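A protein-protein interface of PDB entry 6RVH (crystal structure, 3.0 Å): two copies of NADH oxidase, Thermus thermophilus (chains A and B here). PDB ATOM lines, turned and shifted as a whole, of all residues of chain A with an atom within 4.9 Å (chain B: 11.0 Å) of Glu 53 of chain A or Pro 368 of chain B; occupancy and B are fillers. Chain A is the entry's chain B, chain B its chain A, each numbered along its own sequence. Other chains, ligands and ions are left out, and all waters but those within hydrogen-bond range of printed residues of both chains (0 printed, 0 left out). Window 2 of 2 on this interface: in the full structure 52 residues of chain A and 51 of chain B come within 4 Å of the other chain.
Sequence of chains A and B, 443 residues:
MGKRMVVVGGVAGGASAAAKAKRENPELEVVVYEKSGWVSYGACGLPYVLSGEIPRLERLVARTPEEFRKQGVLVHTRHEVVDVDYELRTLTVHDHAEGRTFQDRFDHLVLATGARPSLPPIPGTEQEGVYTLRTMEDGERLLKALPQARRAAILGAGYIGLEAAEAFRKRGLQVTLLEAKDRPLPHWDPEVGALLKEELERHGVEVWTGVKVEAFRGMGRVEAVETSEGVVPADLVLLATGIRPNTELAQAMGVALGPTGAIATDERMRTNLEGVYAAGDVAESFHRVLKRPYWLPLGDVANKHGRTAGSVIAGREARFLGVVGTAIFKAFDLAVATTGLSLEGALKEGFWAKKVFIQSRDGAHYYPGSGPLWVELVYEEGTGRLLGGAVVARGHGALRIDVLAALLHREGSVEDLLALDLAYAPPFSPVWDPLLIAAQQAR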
ATOM      1  N   TYR A  48      19.213  17.079   2.749  1.00  0.00           N
ATOM      2  CA  TYR A  48      20.254  17.013   1.686  1.00  0.00           C
ATOM      3  C   TYR A  48      21.756  16.802   2.201  1.00  0.00           C
ATOM      4  O   TYR A  48      22.684  16.346   1.412  1.00  0.00           O
ATOM      5  CB  TYR A  48      20.021  18.074   0.617  1.00  0.00           C
ATOM      6  CG  TYR A  48      18.583  17.986   0.233  1.00  0.00           C
ATOM      7  CD1 TYR A  48      18.162  16.951  -0.548  1.00  0.00           C
ATOM      8  CD2 TYR A  48      17.633  18.907   0.721  1.00  0.00           C
ATOM      9  CE1 TYR A  48      16.856  16.837  -0.899  1.00  0.00           C
ATOM     10  CE2 TYR A  48      16.326  18.820   0.400  1.00  0.00           C
ATOM     11  CZ  TYR A  48      15.904  17.774  -0.433  1.00  0.00           C
ATOM     12  OH  TYR A  48      14.516  17.624  -0.775  1.00  0.00           O
ATOM     13  N   SER A  51      21.936  12.908   3.304  1.00  0.00           N
ATOM     14  CA  SER A  51      22.020  12.145   2.070  1.00  0.00           C
ATOM     15  C   SER A  51      23.404  12.250   1.424  1.00  0.00           C
ATOM     16  O   SER A  51      23.722  11.462   0.550  1.00  0.00           O
ATOM     17  CB  SER A  51      20.936  12.679   1.104  1.00  0.00           C
ATOM     18  OG  SER A  51      21.286  13.933   0.504  1.00  0.00           O
ATOM     19  N   GLY A  52      24.211  13.231   1.839  1.00  0.00           N
ATOM     20  CA  GLY A  52      25.542  13.369   1.282  1.00  0.00           C
ATOM     21  C   GLY A  52      25.621  14.248   0.036  1.00  0.00           C
ATOM     22  O   GLY A  52      26.749  14.673  -0.369  1.00  0.00           O
ATOM     23  N   GLU A  53      24.459  14.534  -0.568  1.00  0.00           N
ATOM     24  CA  GLU A  53      24.399  15.462  -1.707  1.00  0.00           C
ATOM     25  C   GLU A  53      25.175  16.794  -1.411  1.00  0.00           C
ATOM     26  O   GLU A  53      25.928  17.348  -2.275  1.00  0.00           O
ATOM     27  CB  GLU A  53      22.921  15.686  -2.149  1.00  0.00           C
ATOM     28  CG  GLU A  53      22.241  14.625  -3.101  1.00  0.00           C
ATOM     29  CD  GLU A  53      20.700  14.711  -3.093  1.00  0.00           C
ATOM     30  OE1 GLU A  53      20.114  15.404  -3.979  1.00  0.00           O
ATOM     31  OE2 GLU A  53      20.070  14.102  -2.179  1.00  0.00           O
ATOM     32  N   ILE A  54      24.993  17.287  -0.185  1.00  0.00           N
ATOM     33  CA  ILE A  54      25.710  18.478   0.260  1.00  0.00           C
ATOM     34  C   ILE A  54      26.763  18.045   1.216  1.00  0.00           C
ATOM     35  O   ILE A  54      26.439  17.577   2.277  1.00  0.00           O
ATOM     36  CB  ILE A  54      24.776  19.506   0.984  1.00  0.00           C
ATOM     37  CG1 ILE A  54      23.635  19.949   0.058  1.00  0.00           C
ATOM     38  CG2 ILE A  54      25.581  20.703   1.502  1.00  0.00           C
ATOM     39  CD1 ILE A  54      22.576  20.676   0.752  1.00  0.00           C
ATOM     40  N   PRO A  55      28.024  18.235   0.862  1.00  0.00           N
ATOM     41  CA  PRO A  55      29.287  17.919   1.566  1.00  0.00           C
ATOM     42  C   PRO A  55      29.293  18.207   3.079  1.00  0.00           C
ATOM     43  O   PRO A  55      29.085  17.272   3.792  1.00  0.00           O
ATOM     44  CB  PRO A  55      30.323  18.843   0.861  1.00  0.00           C
ATOM     45  CG  PRO A  55      29.530  19.963   0.225  1.00  0.00           C
ATOM     46  CD  PRO A  55      28.248  19.209  -0.225  1.00  0.00           C
ATOM     47  N   GLU A 166      14.236   9.331   1.556  1.00  0.00           N
ATOM     48  CA  GLU A 166      15.147   9.524   0.398  1.00  0.00           C
ATOM     49  C   GLU A 166      16.610   9.565   0.904  1.00  0.00           C
ATOM     50  O   GLU A 166      17.563   8.855   0.402  1.00  0.00           O
ATOM     51  CB  GLU A 166      14.848  10.827  -0.396  1.00  0.00           C
ATOM     52  CG  GLU A 166      15.675  11.020  -1.729  1.00  0.00           C
ATOM     53  CD  GLU A 166      15.585  12.487  -2.254  1.00  0.00           C
ATOM     54  OE1 GLU A 166      14.462  12.956  -2.638  1.00  0.00           O
ATOM     55  OE2 GLU A 166      16.650  13.167  -2.251  1.00  0.00           O
ATOM     56  N   LYS A 170      19.619   7.053   0.083  1.00  0.00           N
ATOM     57  CA  LYS A 170      20.812   7.446  -0.685  1.00  0.00           C
ATOM     58  C   LYS A 170      22.117   7.054   0.008  1.00  0.00           C
ATOM     59  O   LYS A 170      23.111   6.821  -0.670  1.00  0.00           O
ATOM     60  CB  LYS A 170      20.826   8.944  -1.038  1.00  0.00           C
ATOM     61  CG  LYS A 170      19.705   9.374  -2.034  1.00  0.00           C
ATOM     62  CD  LYS A 170      19.817  10.850  -2.544  1.00  0.00           C
ATOM     63  CE  LYS A 170      18.634  11.191  -3.450  1.00  0.00           C
ATOM     64  NZ  LYS A 170      18.704  12.469  -4.274  1.00  0.00           N
ATOM     65  N   LYS A 330      10.256  17.376  -1.888  1.00  0.00           N
ATOM     66  CA  LYS A 330      10.837  16.426  -2.902  1.00  0.00           C
ATOM     67  C   LYS A 330      11.139  15.118  -2.306  1.00  0.00           C
ATOM     68  O   LYS A 330      12.040  14.987  -1.529  1.00  0.00           O
ATOM     69  CB  LYS A 330      12.088  17.028  -3.653  1.00  0.00           C
ATOM     70  CG  LYS A 330      12.842  16.246  -4.696  1.00  0.00           C
ATOM     71  CD  LYS A 330      14.387  15.971  -4.266  1.00  0.00           C
ATOM     72  CE  LYS A 330      15.085  14.989  -5.374  1.00  0.00           C
ATOM     73  NZ  LYS A 330      16.307  14.030  -5.191  1.00  0.00           N
ATOM     74  N   ARG B 361      18.075  32.674  -7.593  1.00  0.00           N
ATOM     75  CA  ARG B 361      18.438  31.314  -7.947  1.00  0.00           C
ATOM     76  C   ARG B 361      17.158  30.469  -8.186  1.00  0.00           C
ATOM     77  O   ARG B 361      16.007  30.965  -7.914  1.00  0.00           O
ATOM     78  CB  ARG B 361      19.356  30.664  -6.889  1.00  0.00           C
ATOM     79  CG  ARG B 361      20.553  31.435  -6.551  1.00  0.00           C
ATOM     80  CD  ARG B 361      21.217  30.985  -5.222  1.00  0.00           C
ATOM     81  NE  ARG B 361      22.688  31.023  -5.294  1.00  0.00           N
ATOM     82  CZ  ARG B 361      23.409  30.219  -6.084  1.00  0.00           C
ATOM     83  NH1 ARG B 361      22.780  29.306  -6.877  1.00  0.00           N
ATOM     84  NH2 ARG B 361      24.753  30.335  -6.078  1.00  0.00           N
ATOM     85  N   ASP B 362      17.389  29.212  -8.637  1.00  0.00           N
ATOM     86  CA  ASP B 362      16.351  28.265  -8.811  1.00  0.00           C
ATOM     87  C   ASP B 362      16.461  27.192  -7.787  1.00  0.00           C
ATOM     88  O   ASP B 362      16.403  26.068  -8.143  1.00  0.00           O
ATOM     89  CB  ASP B 362      16.458  27.659 -10.158  1.00  0.00           C
ATOM     90  CG  ASP B 362      15.107  27.140 -10.657  1.00  0.00           C
ATOM     91  OD1 ASP B 362      14.300  26.575  -9.822  1.00  0.00           O
ATOM     92  OD2 ASP B 362      14.877  27.283 -11.901  1.00  0.00           O
ATOM     93  N   GLY B 363      16.567  27.529  -6.503  1.00  0.00           N
ATOM     94  CA  GLY B 363      16.810  26.610  -5.397  1.00  0.00           C
ATOM     95  C   GLY B 363      17.661  27.246  -4.299  1.00  0.00           C
ATOM     96  O   GLY B 363      18.266  28.259  -4.488  1.00  0.00           O
ATOM     97  N   ALA B 364      17.716  26.668  -3.127  1.00  0.00           N
ATOM     98  CA  ALA B 364      18.461  27.326  -2.083  1.00  0.00           C
ATOM     99  C   ALA B 364      19.947  27.547  -2.512  1.00  0.00           C
ATOM    100  O   ALA B 364      20.483  26.729  -3.279  1.00  0.00           O
ATOM    101  CB  ALA B 364      18.346  26.567  -0.750  1.00  0.00           C
ATOM    102  N   HIS B 365      20.600  28.655  -2.064  1.00  0.00           N
ATOM    103  CA  HIS B 365      22.064  28.856  -2.304  1.00  0.00           C
ATOM    104  C   HIS B 365      22.840  27.542  -2.238  1.00  0.00           C
ATOM    105  O   HIS B 365      23.629  27.240  -3.073  1.00  0.00           O
ATOM    106  CB  HIS B 365      22.751  29.997  -1.447  1.00  0.00           C
ATOM    107  CG  HIS B 365      22.878  29.732   0.041  1.00  0.00           C
ATOM    108  ND1 HIS B 365      21.830  29.907   0.941  1.00  0.00           N
ATOM    109  CD2 HIS B 365      23.936  29.354   0.800  1.00  0.00           C
ATOM    110  CE1 HIS B 365      22.219  29.599   2.166  1.00  0.00           C
ATOM    111  NE2 HIS B 365      23.494  29.260   2.108  1.00  0.00           N
ATOM    112  N   TYR B 366      22.533  26.737  -1.249  1.00  0.00           N
ATOM    113  CA  TYR B 366      23.318  25.599  -0.861  1.00  0.00           C
ATOM    114  C   TYR B 366      22.957  24.380  -1.641  1.00  0.00           C
ATOM    115  O   TYR B 366      23.497  23.314  -1.355  1.00  0.00           O
ATOM    116  CB  TYR B 366      23.168  25.249   0.697  1.00  0.00           C
ATOM    117  CG  TYR B 366      21.830  25.001   1.239  1.00  0.00           C
ATOM    118  CD1 TYR B 366      21.268  23.721   1.228  1.00  0.00           C
ATOM    119  CD2 TYR B 366      21.107  26.080   1.770  1.00  0.00           C
ATOM    120  CE1 TYR B 366      19.909  23.537   1.735  1.00  0.00           C
ATOM    121  CE2 TYR B 366      19.800  25.961   2.257  1.00  0.00           C
ATOM    122  CZ  TYR B 366      19.204  24.695   2.263  1.00  0.00           C
ATOM    123  OH  TYR B 366      17.943  24.660   2.790  1.00  0.00           O
ATOM    124  N   TYR B 367      21.981  24.449  -2.541  1.00  0.00           N
ATOM    125  CA  TYR B 367      21.447  23.166  -3.060  1.00  0.00           C
ATOM    126  C   TYR B 367      22.136  22.865  -4.358  1.00  0.00           C
ATOM    127  O   TYR B 367      22.286  23.786  -5.205  1.00  0.00           O
ATOM    128  CB  TYR B 367      19.912  23.107  -3.194  1.00  0.00           C
ATOM    129  CG  TYR B 367      19.246  21.728  -3.573  1.00  0.00           C
ATOM    130  CD1 TYR B 367      18.737  20.832  -2.577  1.00  0.00           C
ATOM    131  CD2 TYR B 367      19.084  21.366  -4.923  1.00  0.00           C
ATOM    132  CE1 TYR B 367      18.147  19.652  -2.921  1.00  0.00           C
ATOM    133  CE2 TYR B 367      18.462  20.185  -5.266  1.00  0.00           C
ATOM    134  CZ  TYR B 367      18.001  19.344  -4.242  1.00  0.00           C
ATOM    135  OH  TYR B 367      17.389  18.147  -4.498  1.00  0.00           O
ATOM    136  N   PRO B 368      22.628  21.607  -4.472  1.00  0.00           N
ATOM    137  CA  PRO B 368      23.359  21.071  -5.606  1.00  0.00           C
ATOM    138  C   PRO B 368      22.683  21.388  -6.941  1.00  0.00           C
ATOM    139  O   PRO B 368      21.495  21.077  -7.092  1.00  0.00           O
ATOM    140  CB  PRO B 368      23.272  19.595  -5.346  1.00  0.00           C
ATOM    141  CG  PRO B 368      23.296  19.521  -3.848  1.00  0.00           C
ATOM    142  CD  PRO B 368      22.606  20.661  -3.341  1.00  0.00           C
ATOM    143  N   GLY B 369      23.414  21.989  -7.880  1.00  0.00           N
ATOM    144  CA  GLY B 369      22.945  22.204  -9.213  1.00  0.00           C
ATOM    145  C   GLY B 369      21.907  23.280  -9.339  1.00  0.00           C
ATOM    146  O   GLY B 369      21.233  23.318 -10.366  1.00  0.00           O
ATOM    147  N   SER B 370      21.775  24.156  -8.328  1.00  0.00           N
ATOM    148  CA  SER B 370      20.717  25.188  -8.295  1.00  0.00           C
ATOM    149  C   SER B 370      21.176  26.121  -9.317  1.00  0.00           C
ATOM    150  O   SER B 370      22.354  26.433  -9.349  1.00  0.00           O
ATOM    151  CB  SER B 370      20.617  25.892  -6.917  1.00  0.00           C
ATOM    152  OG  SER B 370      21.789  26.655  -6.593  1.00  0.00           O
ATOM    153  N   GLY B 371      20.296  26.532 -10.213  1.00  0.00           N
ATOM    154  CA  GLY B 371      20.751  27.458 -11.266  1.00  0.00           C
ATOM    155  C   GLY B 371      20.559  28.936 -10.917  1.00  0.00           C
ATOM    156  O   GLY B 371      20.163  29.290  -9.794  1.00  0.00           O
ATOM    157  N   PRO B 372      20.838  29.822 -11.869  1.00  0.00           N
ATOM    158  CA  PRO B 372      20.326  31.204 -11.763  1.00  0.00           C
ATOM    159  C   PRO B 372      18.905  31.229 -12.242  1.00  0.00           C
ATOM    160  O   PRO B 372      18.380  30.250 -12.853  1.00  0.00           O
ATOM    161  CB  PRO B 372      21.202  31.983 -12.717  1.00  0.00           C
ATOM    162  CG  PRO B 372      21.491  30.998 -13.750  1.00  0.00           C
ATOM    163  CD  PRO B 372      21.568  29.605 -13.122  1.00  0.00           C
ATOM    164  N   ARG B 394      17.155  28.203 -16.202  1.00  0.00           N
ATOM    165  CA  ARG B 394      17.517  27.004 -16.952  1.00  0.00           C
ATOM    166  C   ARG B 394      16.209  26.180 -16.921  1.00  0.00           C
ATOM    167  O   ARG B 394      15.839  25.603 -17.932  1.00  0.00           O
ATOM    168  CB  ARG B 394      18.725  26.230 -16.354  1.00  0.00           C
ATOM    169  CG  ARG B 394      19.821  27.117 -15.710  1.00  0.00           C
ATOM    170  CD  ARG B 394      21.273  26.759 -16.081  1.00  0.00           C
ATOM    171  NE  ARG B 394      22.198  27.935 -15.988  1.00  0.00           N
ATOM    172  CZ  ARG B 394      22.513  28.828 -16.991  1.00  0.00           C
ATOM    173  NH1 ARG B 394      21.965  28.725 -18.197  1.00  0.00           N
ATOM    174  NH2 ARG B 394      23.381  29.864 -16.844  1.00  0.00           N
ATOM    175  N   ALA B 425      10.854  25.209  -1.188  1.00  0.00           N
ATOM    176  CA  ALA B 425      11.674  24.113  -0.647  1.00  0.00           C
ATOM    177  C   ALA B 425      12.930  24.068  -1.413  1.00  0.00           C
ATOM    178  O   ALA B 425      12.944  24.441  -2.590  1.00  0.00           O
ATOM    179  CB  ALA B 425      11.035  22.821  -0.746  1.00  0.00           C
ATOM    180  N   PRO B 426      13.996  23.579  -0.748  1.00  0.00           N
ATOM    181  CA  PRO B 426      15.346  23.893  -1.156  1.00  0.00           C
ATOM    182  C   PRO B 426      15.646  23.595  -2.635  1.00  0.00           C
ATOM    183  O   PRO B 426      16.371  24.299  -3.228  1.00  0.00           O
ATOM    184  CB  PRO B 426      16.166  23.155  -0.107  1.00  0.00           C
ATOM    185  CG  PRO B 426      15.397  23.177   1.005  1.00  0.00           C
ATOM    186  CD  PRO B 426      14.008  22.931   0.566  1.00  0.00           C
ATOM    187  N   PRO B 427      15.065  22.556  -3.222  1.00  0.00           N
ATOM    188  CA  PRO B 427      15.441  22.224  -4.604  1.00  0.00           C
ATOM    189  C   PRO B 427      14.837  23.103  -5.674  1.00  0.00           C
ATOM    190  O   PRO B 427      15.236  22.984  -6.836  1.00  0.00           O
ATOM    191  CB  PRO B 427      14.843  20.852  -4.755  1.00  0.00           C
ATOM    192  CG  PRO B 427      14.748  20.281  -3.367  1.00  0.00           C
ATOM    193  CD  PRO B 427      14.470  21.400  -2.482  1.00  0.00           C
ATOM    194  N   PHE B 428      13.859  23.949  -5.303  1.00  0.00           N
ATOM    195  CA  PHE B 428      12.985  24.553  -6.287  1.00  0.00           C
ATOM    196  C   PHE B 428      12.992  26.028  -6.185  1.00  0.00           C
ATOM    197  O   PHE B 428      12.596  26.746  -7.112  1.00  0.00           O
ATOM    198  CB  PHE B 428      11.561  24.088  -6.141  1.00  0.00           C
ATOM    199  CG  PHE B 428      11.408  22.616  -6.076  1.00  0.00           C
ATOM    200  CD1 PHE B 428      11.934  21.801  -7.045  1.00  0.00           C
ATOM    201  CD2 PHE B 428      10.780  22.012  -5.004  1.00  0.00           C
ATOM    202  CE1 PHE B 428      11.825  20.418  -6.946  1.00  0.00           C
ATOM    203  CE2 PHE B 428      10.638  20.614  -4.932  1.00  0.00           C
ATOM    204  CZ  PHE B 428      11.178  19.843  -5.882  1.00  0.00           C
ATOM    205  N   SER B 429      13.478  26.526  -5.073  1.00  0.00           N
ATOM    206  CA  SER B 429      13.336  27.985  -4.863  1.00  0.00           C
ATOM    207  C   SER B 429      14.161  28.369  -3.648  1.00  0.00           C
ATOM    208  O   SER B 429      14.208  27.613  -2.698  1.00  0.00           O
ATOM    209  CB  SER B 429      11.812  28.337  -4.658  1.00  0.00           C
ATOM    210  OG  SER B 429      11.493  29.716  -4.527  1.00  0.00           O
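NZ of Lys 330 of chain A lies within salt-bridge range of OE2 of Glu 166 of chain A. The backbone carbonyl oxygen of Tyr 48 of chain A lies within hydrogen-bond range of the side-chain hydroxyl of Ser 51 of chain A (2.9 Å). O of Tyr 367 of chain B sits close to OG of Ser 370 of chain B. N of Glu 53 of chain A lies within hydrogen-bond range of O of Tyr 48 of chain A (3.2 Å). OE2 of Glu 53 of chain A is in hydrogen-bond range of OG of Ser 51 of chain A, at 3.0 Å. The backbone carbonyl oxygen (O) of Tyr 48 of chain A sits at hydrogen-bond distance from the backbone NH (N) of Ile 54 of chain A (3.0 Å).
Among the printed residues, pairs that only touch across the chains: Tyr 48 of chain A with Tyr 367 of chain B (3.6 Å), Tyr 48 of chain A with Pro 427 of chain B (3.7 Å), Glu 53 of chain A with Tyr 367 of chain B (3.9 Å), Glu 53 of chain A with Pro 368 of chain B (3.8 Å), Ile 54 of chain A with Tyr 366 of chain B (3.3 Å), Ile 54 of chain A with Pro 368 of chain B (3.6 Å), Lys 330 of chain A with Tyr 367 of chain B (3.7 Å) and Lys 330 of chain A with Phe 428 of chain B (3.7 Å).
Tyr 48 of chain A touches two residues of chain B. No residue of chain B comes within 4 Å of Gly 52 of chain A. Of chain B, only Tyr 367 and Pro 368 come within 4 Å of Glu 53 of chain A. Ile 54 of chain A touches just these residues of chain B: Tyr 366 (3.3 Å) and Pro 368 (3.6 Å). Pro 55 of chain A touches none of the printed residues of chain B. Ala 364 of chain B touches none of the printed residues of chain A. Of the printed residues of chain A, Tyr 366 of chain B touches Ile 54 (3.3 Å). Pro 368 of chain B touches just these residues of chain A: Glu 53 and Ile 54. Pro 372 of chain B touches none of the printed residues of chain A. Of the printed residues of chain A, Pro 427 of chain B touches Tyr 48. Of the printed residues of chain A, Phe 428 of chain B touches Lys 330 (3.7 Å). The nearest residue of chain B that does not touch Glu 53 of chain A is Tyr 366 of chain B (6.5 Å).
Printed residues of chain B that touch a printed residue of chain A: Tyr 366, Tyr 367, Pro 368, Pro 427 and Phe 428. Of the 9 printed residues of chain A, 4 touch a printed residue of chain B. Printed residues of chain A that touch a printed residue of chain B: Tyr 48, Glu 53, Ile 54 and Lys 330. Among the printed residues, no Asp or Glu carboxylate lies within 4 Å of a Lys or Arg side-chain nitrogen of the other chain.
No position is printed for both chains.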
